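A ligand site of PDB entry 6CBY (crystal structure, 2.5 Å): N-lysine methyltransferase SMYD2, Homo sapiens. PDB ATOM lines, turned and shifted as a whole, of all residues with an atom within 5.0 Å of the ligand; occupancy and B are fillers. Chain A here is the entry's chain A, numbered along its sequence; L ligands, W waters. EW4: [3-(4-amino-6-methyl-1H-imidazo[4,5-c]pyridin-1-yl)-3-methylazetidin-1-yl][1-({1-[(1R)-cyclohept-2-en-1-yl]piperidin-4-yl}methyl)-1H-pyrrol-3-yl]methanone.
A ring nitrogen (NE2) of His 138 sits at hydrogen-bond distance from the backbone carbonyl oxygen of Tyr 259 (3.1 Å).
N of Tyr 241 is in hydrogen-bond range of ND1 of His 208 (2.9 Å).
NE2 of His 208 lies close to SG of Cys 263, 3.6 Å away.
The side-chain carboxylate of Glu 264 is in salt-bridge range of the side-chain amino group of Lys 18 (3.7 Å).
The side-chain sulfur (SG) of Cys 182 sits at hydrogen-bond distance from the side-chain amide nitrogen (ND2) of Asn 183, at 3.4 Å.
SG of Cys 182 is in hydrogen-bond range of O of Glu 136, 3.4 Å away.
OD1 of Asn 207 lies close to O of Arg 20.
O of Glu 136 is in hydrogen-bond range of ND2 of Asn 183, at 2.7 Å.
Water W2 bridges the backbone carbonyl oxygen of Tyr 259 (2.7 Å) and an oxygen (O) of the ligand (3.0 Å).
Water W3 lies within hydrogen-bond range of O of Ala 204 (2.7 Å) and OH of Tyr 241 (3.3 Å).
O of the ligand sits at hydrogen-bond distance from NE2 of His 138 (2.8 Å).
The backbone NH of His 208 lies within hydrogen-bond range of a nitrogen (N4) of the ligand.
O of His 208 lies within hydrogen-bond range of N6 of the ligand (3.0 Å).
The side-chain carboxylate (OE1) of Glu 264 lies within hydrogen-bond range of a nitrogen (N6) of the ligand, 3.0 Å away.
O of the ligand lies close to O of Tyr 259, 3.1 Å away.
O of Gly 17 touches C27 of the ligand (3.5 Å).
O of Lys 18 touches C of the ligand, 3.4 Å away.
O of Cys 182 touches C7 of the ligand (3.2 Å).
O of Asn 183 touches C8 of the ligand, 3.4 Å away.
O of Gly 184 touches C16 of the ligand (3.2 Å).
Phe 185 touches the ligand.
OG1 of Thr 186 touches C14 of the ligand, 3.4 Å away.
Ala 204 touches the ligand (O to C6, 3.9 Å).
OD1 of Asn 207 touches C22 of the ligand, at 3.3 Å.
OH of Tyr 241 touches C22 of the ligand, at 3.4 Å.
Phe 261 touches the ligand (CE1 to C23, 3.4 Å).
Thr 262 touches the ligand.
Hydrophobic or aromatic side chains within 4 Å of the ligand: His 138, Phe 185, His 208, Tyr 241, Tyr 259 and Phe 261.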
ATOM      1  N   GLY A  17      -3.981  34.439 -28.704  1.00  0.00           N
ATOM      2  CA  GLY A  17      -3.951  32.994 -28.834  1.00  0.00           C
ATOM      3  C   GLY A  17      -2.815  32.314 -28.129  1.00  0.00           C
ATOM      4  O   GLY A  17      -2.737  31.086 -28.174  1.00  0.00           O
ATOM      5  N   LYS A  18      -1.905  33.100 -27.478  1.00  0.00           N
ATOM      6  CA  LYS A  18      -0.698  32.593 -26.776  1.00  0.00           C
ATOM      7  C   LYS A  18      -0.608  33.109 -25.331  1.00  0.00           C
ATOM      8  O   LYS A  18      -0.818  32.349 -24.398  1.00  0.00           O
ATOM      9  CB  LYS A  18       0.599  32.965 -27.536  1.00  0.00           C
ATOM     10  CG  LYS A  18       0.642  32.574 -29.012  1.00  0.00           C
ATOM     11  CD  LYS A  18       1.834  33.252 -29.720  1.00  0.00           C
ATOM     12  CE  LYS A  18       2.025  32.819 -31.150  1.00  0.00           C
ATOM     13  NZ  LYS A  18       0.806  33.010 -31.988  1.00  0.00           N
ATOM     14  N   GLY A  19      -0.322  34.379 -25.143  1.00  0.00           N
ATOM     15  CA  GLY A  19      -0.206  34.961 -23.810  1.00  0.00           C
ATOM     16  C   GLY A  19       0.873  36.001 -23.780  1.00  0.00           C
ATOM     17  O   GLY A  19       1.130  36.641 -24.793  1.00  0.00           O
ATOM     18  N   ARG A  20       1.566  36.140 -22.639  1.00  0.00           N
ATOM     19  CA  ARG A  20       2.656  37.090 -22.395  1.00  0.00           C
ATOM     20  C   ARG A  20       3.777  36.907 -23.432  1.00  0.00           C
ATOM     21  O   ARG A  20       4.269  35.786 -23.616  1.00  0.00           O
ATOM     22  CB  ARG A  20       3.206  36.911 -20.967  1.00  0.00           C
ATOM     23  CG  ARG A  20       2.165  37.042 -19.867  1.00  0.00           C
ATOM     24  CD  ARG A  20       2.686  36.729 -18.468  1.00  0.00           C
ATOM     25  NE  ARG A  20       3.318  35.414 -18.361  1.00  0.00           N
ATOM     26  CZ  ARG A  20       3.844  34.927 -17.244  1.00  0.00           C
ATOM     27  NH1 ARG A  20       3.810  35.633 -16.122  1.00  0.00           N
ATOM     28  NH2 ARG A  20       4.405  33.726 -17.238  1.00  0.00           N
ATOM     29  N   GLU A 136       5.530  30.538 -15.030  1.00  0.00           N
ATOM     30  CA  GLU A 136       4.566  29.477 -15.235  1.00  0.00           C
ATOM     31  C   GLU A 136       5.172  28.206 -14.620  1.00  0.00           C
ATOM     32  O   GLU A 136       6.354  27.908 -14.763  1.00  0.00           O
ATOM     33  CB  GLU A 136       4.268  29.320 -16.727  1.00  0.00           C
ATOM     34  CG  GLU A 136       3.350  28.167 -17.090  1.00  0.00           C
ATOM     35  CD  GLU A 136       1.926  28.201 -16.559  1.00  0.00           C
ATOM     36  OE1 GLU A 136       1.149  29.081 -16.995  1.00  0.00           O
ATOM     37  OE2 GLU A 136       1.573  27.332 -15.733  1.00  0.00           O
ATOM     38  N   HIS A 138       2.933  25.155 -14.612  1.00  0.00           N
ATOM     39  CA  HIS A 138       2.129  24.073 -15.249  1.00  0.00           C
ATOM     40  C   HIS A 138       1.868  22.874 -14.288  1.00  0.00           C
ATOM     41  O   HIS A 138       1.781  21.731 -14.742  1.00  0.00           O
ATOM     42  CB  HIS A 138       2.784  23.536 -16.539  1.00  0.00           C
ATOM     43  CG  HIS A 138       2.859  24.498 -17.679  1.00  0.00           C
ATOM     44  ND1 HIS A 138       1.725  25.094 -18.220  1.00  0.00           N
ATOM     45  CD2 HIS A 138       3.925  24.846 -18.436  1.00  0.00           C
ATOM     46  CE1 HIS A 138       2.141  25.802 -19.247  1.00  0.00           C
ATOM     47  NE2 HIS A 138       3.472  25.697 -19.407  1.00  0.00           N
ATOM     48  N   CYS A 182      10.325  23.945 -16.342  1.00  0.00           N
ATOM     49  CA  CYS A 182       9.912  24.382 -17.680  1.00  0.00           C
ATOM     50  C   CYS A 182      10.461  25.779 -18.024  1.00  0.00           C
ATOM     51  O   CYS A 182      10.484  26.130 -19.198  1.00  0.00           O
ATOM     52  CB  CYS A 182       8.384  24.300 -17.855  1.00  0.00           C
ATOM     53  SG  CYS A 182       7.431  25.444 -16.813  1.00  0.00           S
ATOM     54  N   ASN A 183      10.992  26.525 -17.046  1.00  0.00           N
ATOM     55  CA  ASN A 183      11.544  27.858 -17.323  1.00  0.00           C
ATOM     56  C   ASN A 183      13.093  27.914 -17.410  1.00  0.00           C
ATOM     57  O   ASN A 183      13.596  28.876 -17.962  1.00  0.00           O
ATOM     58  CB  ASN A 183      11.063  28.877 -16.293  1.00  0.00           C
ATOM     59  CG  ASN A 183       9.638  29.321 -16.509  1.00  0.00           C
ATOM     60  OD1 ASN A 183       9.364  30.358 -17.120  1.00  0.00           O
ATOM     61  ND2 ASN A 183       8.701  28.506 -16.048  1.00  0.00           N
ATOM     62  N   GLY A 184      13.796  26.919 -16.845  1.00  0.00           N
ATOM     63  CA  GLY A 184      15.254  26.847 -16.795  1.00  0.00           C
ATOM     64  C   GLY A 184      15.930  26.747 -18.145  1.00  0.00           C
ATOM     65  O   GLY A 184      15.491  25.968 -18.994  1.00  0.00           O
ATOM     66  N   PHE A 185      16.989  27.529 -18.371  1.00  0.00           N
ATOM     67  CA  PHE A 185      17.760  27.505 -19.617  1.00  0.00           C
ATOM     68  C   PHE A 185      19.000  26.659 -19.452  1.00  0.00           C
ATOM     69  O   PHE A 185      19.612  26.646 -18.387  1.00  0.00           O
ATOM     70  CB  PHE A 185      18.198  28.925 -20.022  1.00  0.00           C
ATOM     71  CG  PHE A 185      17.099  29.740 -20.658  1.00  0.00           C
ATOM     72  CD1 PHE A 185      16.866  29.671 -22.028  1.00  0.00           C
ATOM     73  CD2 PHE A 185      16.281  30.545 -19.880  1.00  0.00           C
ATOM     74  CE1 PHE A 185      15.820  30.400 -22.615  1.00  0.00           C
ATOM     75  CE2 PHE A 185      15.242  31.288 -20.454  1.00  0.00           C
ATOM     76  CZ  PHE A 185      15.021  31.205 -21.816  1.00  0.00           C
ATOM     77  N   THR A 186      19.352  25.930 -20.492  1.00  0.00           N
ATOM     78  CA  THR A 186      20.588  25.157 -20.558  1.00  0.00           C
ATOM     79  C   THR A 186      21.505  26.111 -21.344  1.00  0.00           C
ATOM     80  O   THR A 186      21.034  26.788 -22.274  1.00  0.00           O
ATOM     81  CB  THR A 186      20.400  23.829 -21.321  1.00  0.00           C
ATOM     82  OG1 THR A 186      19.817  24.075 -22.603  1.00  0.00           O
ATOM     83  CG2 THR A 186      19.559  22.794 -20.566  1.00  0.00           C
ATOM     84  N   ALA A 204      12.875  34.354 -20.990  1.00  0.00           N
ATOM     85  CA  ALA A 204      11.742  33.422 -20.847  1.00  0.00           C
ATOM     86  C   ALA A 204      10.397  34.077 -21.296  1.00  0.00           C
ATOM     87  O   ALA A 204       9.479  33.355 -21.670  1.00  0.00           O
ATOM     88  CB  ALA A 204      11.647  32.915 -19.407  1.00  0.00           C
ATOM     89  N   ASN A 207       7.994  34.199 -26.890  1.00  0.00           N
ATOM     90  CA  ASN A 207       7.140  33.102 -27.315  1.00  0.00           C
ATOM     91  C   ASN A 207       7.880  32.262 -28.388  1.00  0.00           C
ATOM     92  O   ASN A 207       8.989  32.622 -28.776  1.00  0.00           O
ATOM     93  CB  ASN A 207       5.749  33.631 -27.777  1.00  0.00           C
ATOM     94  CG  ASN A 207       4.811  33.982 -26.624  1.00  0.00           C
ATOM     95  OD1 ASN A 207       5.031  33.572 -25.463  1.00  0.00           O
ATOM     96  ND2 ASN A 207       3.730  34.753 -26.897  1.00  0.00           N
ATOM     97  N   HIS A 208       7.295  31.120 -28.791  1.00  0.00           N
ATOM     98  CA  HIS A 208       7.901  30.166 -29.707  1.00  0.00           C
ATOM     99  C   HIS A 208       7.407  30.276 -31.166  1.00  0.00           C
ATOM    100  O   HIS A 208       6.242  30.582 -31.428  1.00  0.00           O
ATOM    101  CB  HIS A 208       7.622  28.745 -29.180  1.00  0.00           C
ATOM    102  CG  HIS A 208       7.919  27.694 -30.191  1.00  0.00           C
ATOM    103  ND1 HIS A 208       9.211  27.260 -30.414  1.00  0.00           N
ATOM    104  CD2 HIS A 208       7.112  27.115 -31.098  1.00  0.00           C
ATOM    105  CE1 HIS A 208       9.134  26.438 -31.447  1.00  0.00           C
ATOM    106  NE2 HIS A 208       7.901  26.320 -31.888  1.00  0.00           N
ATOM    107  N   PHE A 238      10.102  36.132 -31.579  1.00  0.00           N
ATOM    108  CA  PHE A 238      10.049  34.673 -31.467  1.00  0.00           C
ATOM    109  C   PHE A 238      11.404  34.021 -31.521  1.00  0.00           C
ATOM    110  O   PHE A 238      12.220  34.231 -32.436  1.00  0.00           O
ATOM    111  CB  PHE A 238       9.201  34.042 -32.577  1.00  0.00           C
ATOM    112  CG  PHE A 238       7.721  34.323 -32.513  1.00  0.00           C
ATOM    113  CD1 PHE A 238       6.919  33.700 -31.582  1.00  0.00           C
ATOM    114  CD2 PHE A 238       7.119  35.136 -33.461  1.00  0.00           C
ATOM    115  CE1 PHE A 238       5.545  33.910 -31.559  1.00  0.00           C
ATOM    116  CE2 PHE A 238       5.735  35.377 -33.419  1.00  0.00           C
ATOM    117  CZ  PHE A 238       4.953  34.723 -32.496  1.00  0.00           C
ATOM    118  N   SER A 240      12.918  29.816 -30.653  1.00  0.00           N
ATOM    119  CA  SER A 240      12.435  28.447 -30.759  1.00  0.00           C
ATOM    120  C   SER A 240      12.731  27.753 -29.490  1.00  0.00           C
ATOM    121  O   SER A 240      13.876  27.727 -29.021  1.00  0.00           O
ATOM    122  CB  SER A 240      13.060  27.686 -31.920  1.00  0.00           C
ATOM    123  OG  SER A 240      12.777  26.305 -31.759  1.00  0.00           O
ATOM    124  N   TYR A 241      11.689  27.173 -28.915  1.00  0.00           N
ATOM    125  CA  TYR A 241      11.805  26.421 -27.679  1.00  0.00           C
ATOM    126  C   TYR A 241      12.485  25.072 -27.946  1.00  0.00           C
ATOM    127  O   TYR A 241      13.056  24.515 -27.024  1.00  0.00           O
ATOM    128  CB  TYR A 241      10.429  26.191 -27.061  1.00  0.00           C
ATOM    129  CG  TYR A 241       9.757  27.404 -26.420  1.00  0.00           C
ATOM    130  CD1 TYR A 241      10.234  28.694 -26.644  1.00  0.00           C
ATOM    131  CD2 TYR A 241       8.609  27.265 -25.659  1.00  0.00           C
ATOM    132  CE1 TYR A 241       9.587  29.808 -26.111  1.00  0.00           C
ATOM    133  CE2 TYR A 241       7.952  28.369 -25.126  1.00  0.00           C
ATOM    134  CZ  TYR A 241       8.450  29.646 -25.332  1.00  0.00           C
ATOM    135  OH  TYR A 241       7.812  30.691 -24.699  1.00  0.00           O
ATOM    136  N   TYR A 259       5.953  22.099 -22.506  1.00  0.00           N
ATOM    137  CA  TYR A 259       5.286  23.374 -22.258  1.00  0.00           C
ATOM    138  C   TYR A 259       3.772  23.297 -22.446  1.00  0.00           C
ATOM    139  O   TYR A 259       3.091  24.281 -22.159  1.00  0.00           O
ATOM    140  CB  TYR A 259       5.912  24.509 -23.105  1.00  0.00           C
ATOM    141  CG  TYR A 259       7.421  24.414 -23.102  1.00  0.00           C
ATOM    142  CD1 TYR A 259       8.149  24.659 -21.939  1.00  0.00           C
ATOM    143  CD2 TYR A 259       8.110  23.884 -24.201  1.00  0.00           C
ATOM    144  CE1 TYR A 259       9.520  24.433 -21.881  1.00  0.00           C
ATOM    145  CE2 TYR A 259       9.485  23.693 -24.169  1.00  0.00           C
ATOM    146  CZ  TYR A 259      10.190  23.963 -23.004  1.00  0.00           C
ATOM    147  OH  TYR A 259      11.553  23.785 -22.979  1.00  0.00           O
ATOM    148  N   PHE A 261       1.608  23.209 -24.874  1.00  0.00           N
ATOM    149  CA  PHE A 261       0.973  24.015 -25.906  1.00  0.00           C
ATOM    150  C   PHE A 261       1.358  23.400 -27.272  1.00  0.00           C
ATOM    151  O   PHE A 261       2.349  22.688 -27.371  1.00  0.00           O
ATOM    152  CB  PHE A 261       1.389  25.506 -25.788  1.00  0.00           C
ATOM    153  CG  PHE A 261       2.777  25.878 -26.285  1.00  0.00           C
ATOM    154  CD1 PHE A 261       2.991  26.180 -27.627  1.00  0.00           C
ATOM    155  CD2 PHE A 261       3.839  26.006 -25.412  1.00  0.00           C
ATOM    156  CE1 PHE A 261       4.262  26.512 -28.099  1.00  0.00           C
ATOM    157  CE2 PHE A 261       5.110  26.339 -25.885  1.00  0.00           C
ATOM    158  CZ  PHE A 261       5.309  26.605 -27.212  1.00  0.00           C
ATOM    159  N   THR A 262       0.560  23.690 -28.305  1.00  0.00           N
ATOM    160  CA  THR A 262       0.769  23.229 -29.683  1.00  0.00           C
ATOM    161  C   THR A 262       1.037  24.473 -30.526  1.00  0.00           C
ATOM    162  O   THR A 262       0.429  25.522 -30.299  1.00  0.00           O
ATOM    163  CB  THR A 262      -0.450  22.381 -30.110  1.00  0.00           C
ATOM    164  OG1 THR A 262      -0.394  21.133 -29.397  1.00  0.00           O
ATOM    165  CG2 THR A 262      -0.510  22.107 -31.628  1.00  0.00           C
ATOM    166  N   CYS A 263       1.977  24.367 -31.493  1.00  0.00           N
ATOM    167  CA  CYS A 263       2.407  25.453 -32.357  1.00  0.00           C
ATOM    168  C   CYS A 263       1.487  25.613 -33.592  1.00  0.00           C
ATOM    169  O   CYS A 263       0.888  24.667 -34.075  1.00  0.00           O
ATOM    170  CB  CYS A 263       3.864  25.264 -32.769  1.00  0.00           C
ATOM    171  SG  CYS A 263       4.645  26.751 -33.420  1.00  0.00           S
ATOM    172  N   GLU A 264       1.411  26.874 -34.092  1.00  0.00           N
ATOM    173  CA  GLU A 264       0.582  27.297 -35.206  1.00  0.00           C
ATOM    174  C   GLU A 264       1.352  28.167 -36.230  1.00  0.00           C
ATOM    175  O   GLU A 264       0.717  28.823 -37.055  1.00  0.00           O
ATOM    176  CB  GLU A 264      -0.676  28.048 -34.673  1.00  0.00           C
ATOM    177  CG  GLU A 264      -0.443  29.349 -33.904  1.00  0.00           C
ATOM    178  CD  GLU A 264       0.306  29.257 -32.577  1.00  0.00           C
ATOM    179  OE1 GLU A 264       1.545  29.433 -32.619  1.00  0.00           O
ATOM    180  OE2 GLU A 264      -0.324  29.040 -31.516  1.00  0.00           O
HETATM  181  C4  EW4 L   1       5.942  28.320 -21.241  1.00  0.00           C
HETATM  182  C5  EW4 L   1       7.022  29.088 -21.633  1.00  0.00           C
HETATM  183  C6  EW4 L   1       9.354  29.586 -20.777  1.00  0.00           C
HETATM  184  N1  EW4 L   1       8.030  28.936 -20.713  1.00  0.00           N
HETATM  185  C7  EW4 L   1      10.459  28.648 -21.250  1.00  0.00           C
HETATM  186  C8  EW4 L   1      11.883  29.097 -20.918  1.00  0.00           C
HETATM  187  N2  EW4 L   1      12.780  27.663 -22.784  1.00  0.00           N
HETATM  188  C9  EW4 L   1      12.911  28.045 -21.355  1.00  0.00           C
HETATM  189  C10 EW4 L   1      13.738  26.623 -23.213  1.00  0.00           C
HETATM  190  C11 EW4 L   1      14.268  26.973 -24.581  1.00  0.00           C
HETATM  191  C12 EW4 L   1      15.280  26.448 -25.276  1.00  0.00           C
HETATM  192  N3  EW4 L   1       3.661  30.139 -25.767  1.00  0.00           N
HETATM  193  C13 EW4 L   1      16.215  25.329 -24.945  1.00  0.00           C
HETATM  194  C14 EW4 L   1      16.684  25.163 -23.490  1.00  0.00           C
HETATM  195  C15 EW4 L   1      15.533  24.876 -22.539  1.00  0.00           C
HETATM  196  N4  EW4 L   1       4.880  30.233 -27.659  1.00  0.00           N
HETATM  197  O   EW4 L   1       3.910  27.206 -21.686  1.00  0.00           O
HETATM  198  C3  EW4 L   1       4.617  28.184 -21.925  1.00  0.00           C
HETATM  199  N   EW4 L   1       4.212  29.149 -22.780  1.00  0.00           N
HETATM  200  C2  EW4 L   1       2.982  29.056 -23.573  1.00  0.00           C
HETATM  201  C21 EW4 L   1       4.681  30.381 -23.432  1.00  0.00           C
HETATM  202  C1  EW4 L   1       3.405  30.354 -24.320  1.00  0.00           C
HETATM  203  C24 EW4 L   1       2.807  29.773 -26.799  1.00  0.00           C
HETATM  204  C25 EW4 L   1       1.484  29.375 -26.820  1.00  0.00           C
HETATM  205  C26 EW4 L   1       0.936  29.022 -28.053  1.00  0.00           C
HETATM  206  C27 EW4 L   1      -0.459  28.495 -28.177  1.00  0.00           C
HETATM  207  N5  EW4 L   1       1.659  29.101 -29.199  1.00  0.00           N
HETATM  208  C28 EW4 L   1       2.959  29.501 -29.186  1.00  0.00           C
HETATM  209  N6  EW4 L   1       3.583  29.550 -30.373  1.00  0.00           N
HETATM  210  C23 EW4 L   1       3.577  29.842 -27.960  1.00  0.00           C
HETATM  211  C22 EW4 L   1       4.877  30.394 -26.361  1.00  0.00           C
HETATM  212  C   EW4 L   1       2.496  31.544 -24.076  1.00  0.00           C
HETATM  213  C20 EW4 L   1       6.331  27.672 -20.021  1.00  0.00           C
HETATM  214  C19 EW4 L   1       7.598  28.079 -19.736  1.00  0.00           C
HETATM  215  C18 EW4 L   1      10.374  28.339 -22.734  1.00  0.00           C
HETATM  216  C17 EW4 L   1      11.395  27.286 -23.134  1.00  0.00           C
HETATM  217  C16 EW4 L   1      14.699  26.092 -22.143  1.00  0.00           C
HETATM  218  O   HOH W   1      13.196  29.886 -24.728  1.00  0.00           O
HETATM  219  O   HOH W   2       1.213  26.192 -22.409  1.00  0.00           O
HETATM  220  O   HOH W   3       6.925  32.765 -22.315  1.00  0.00           O
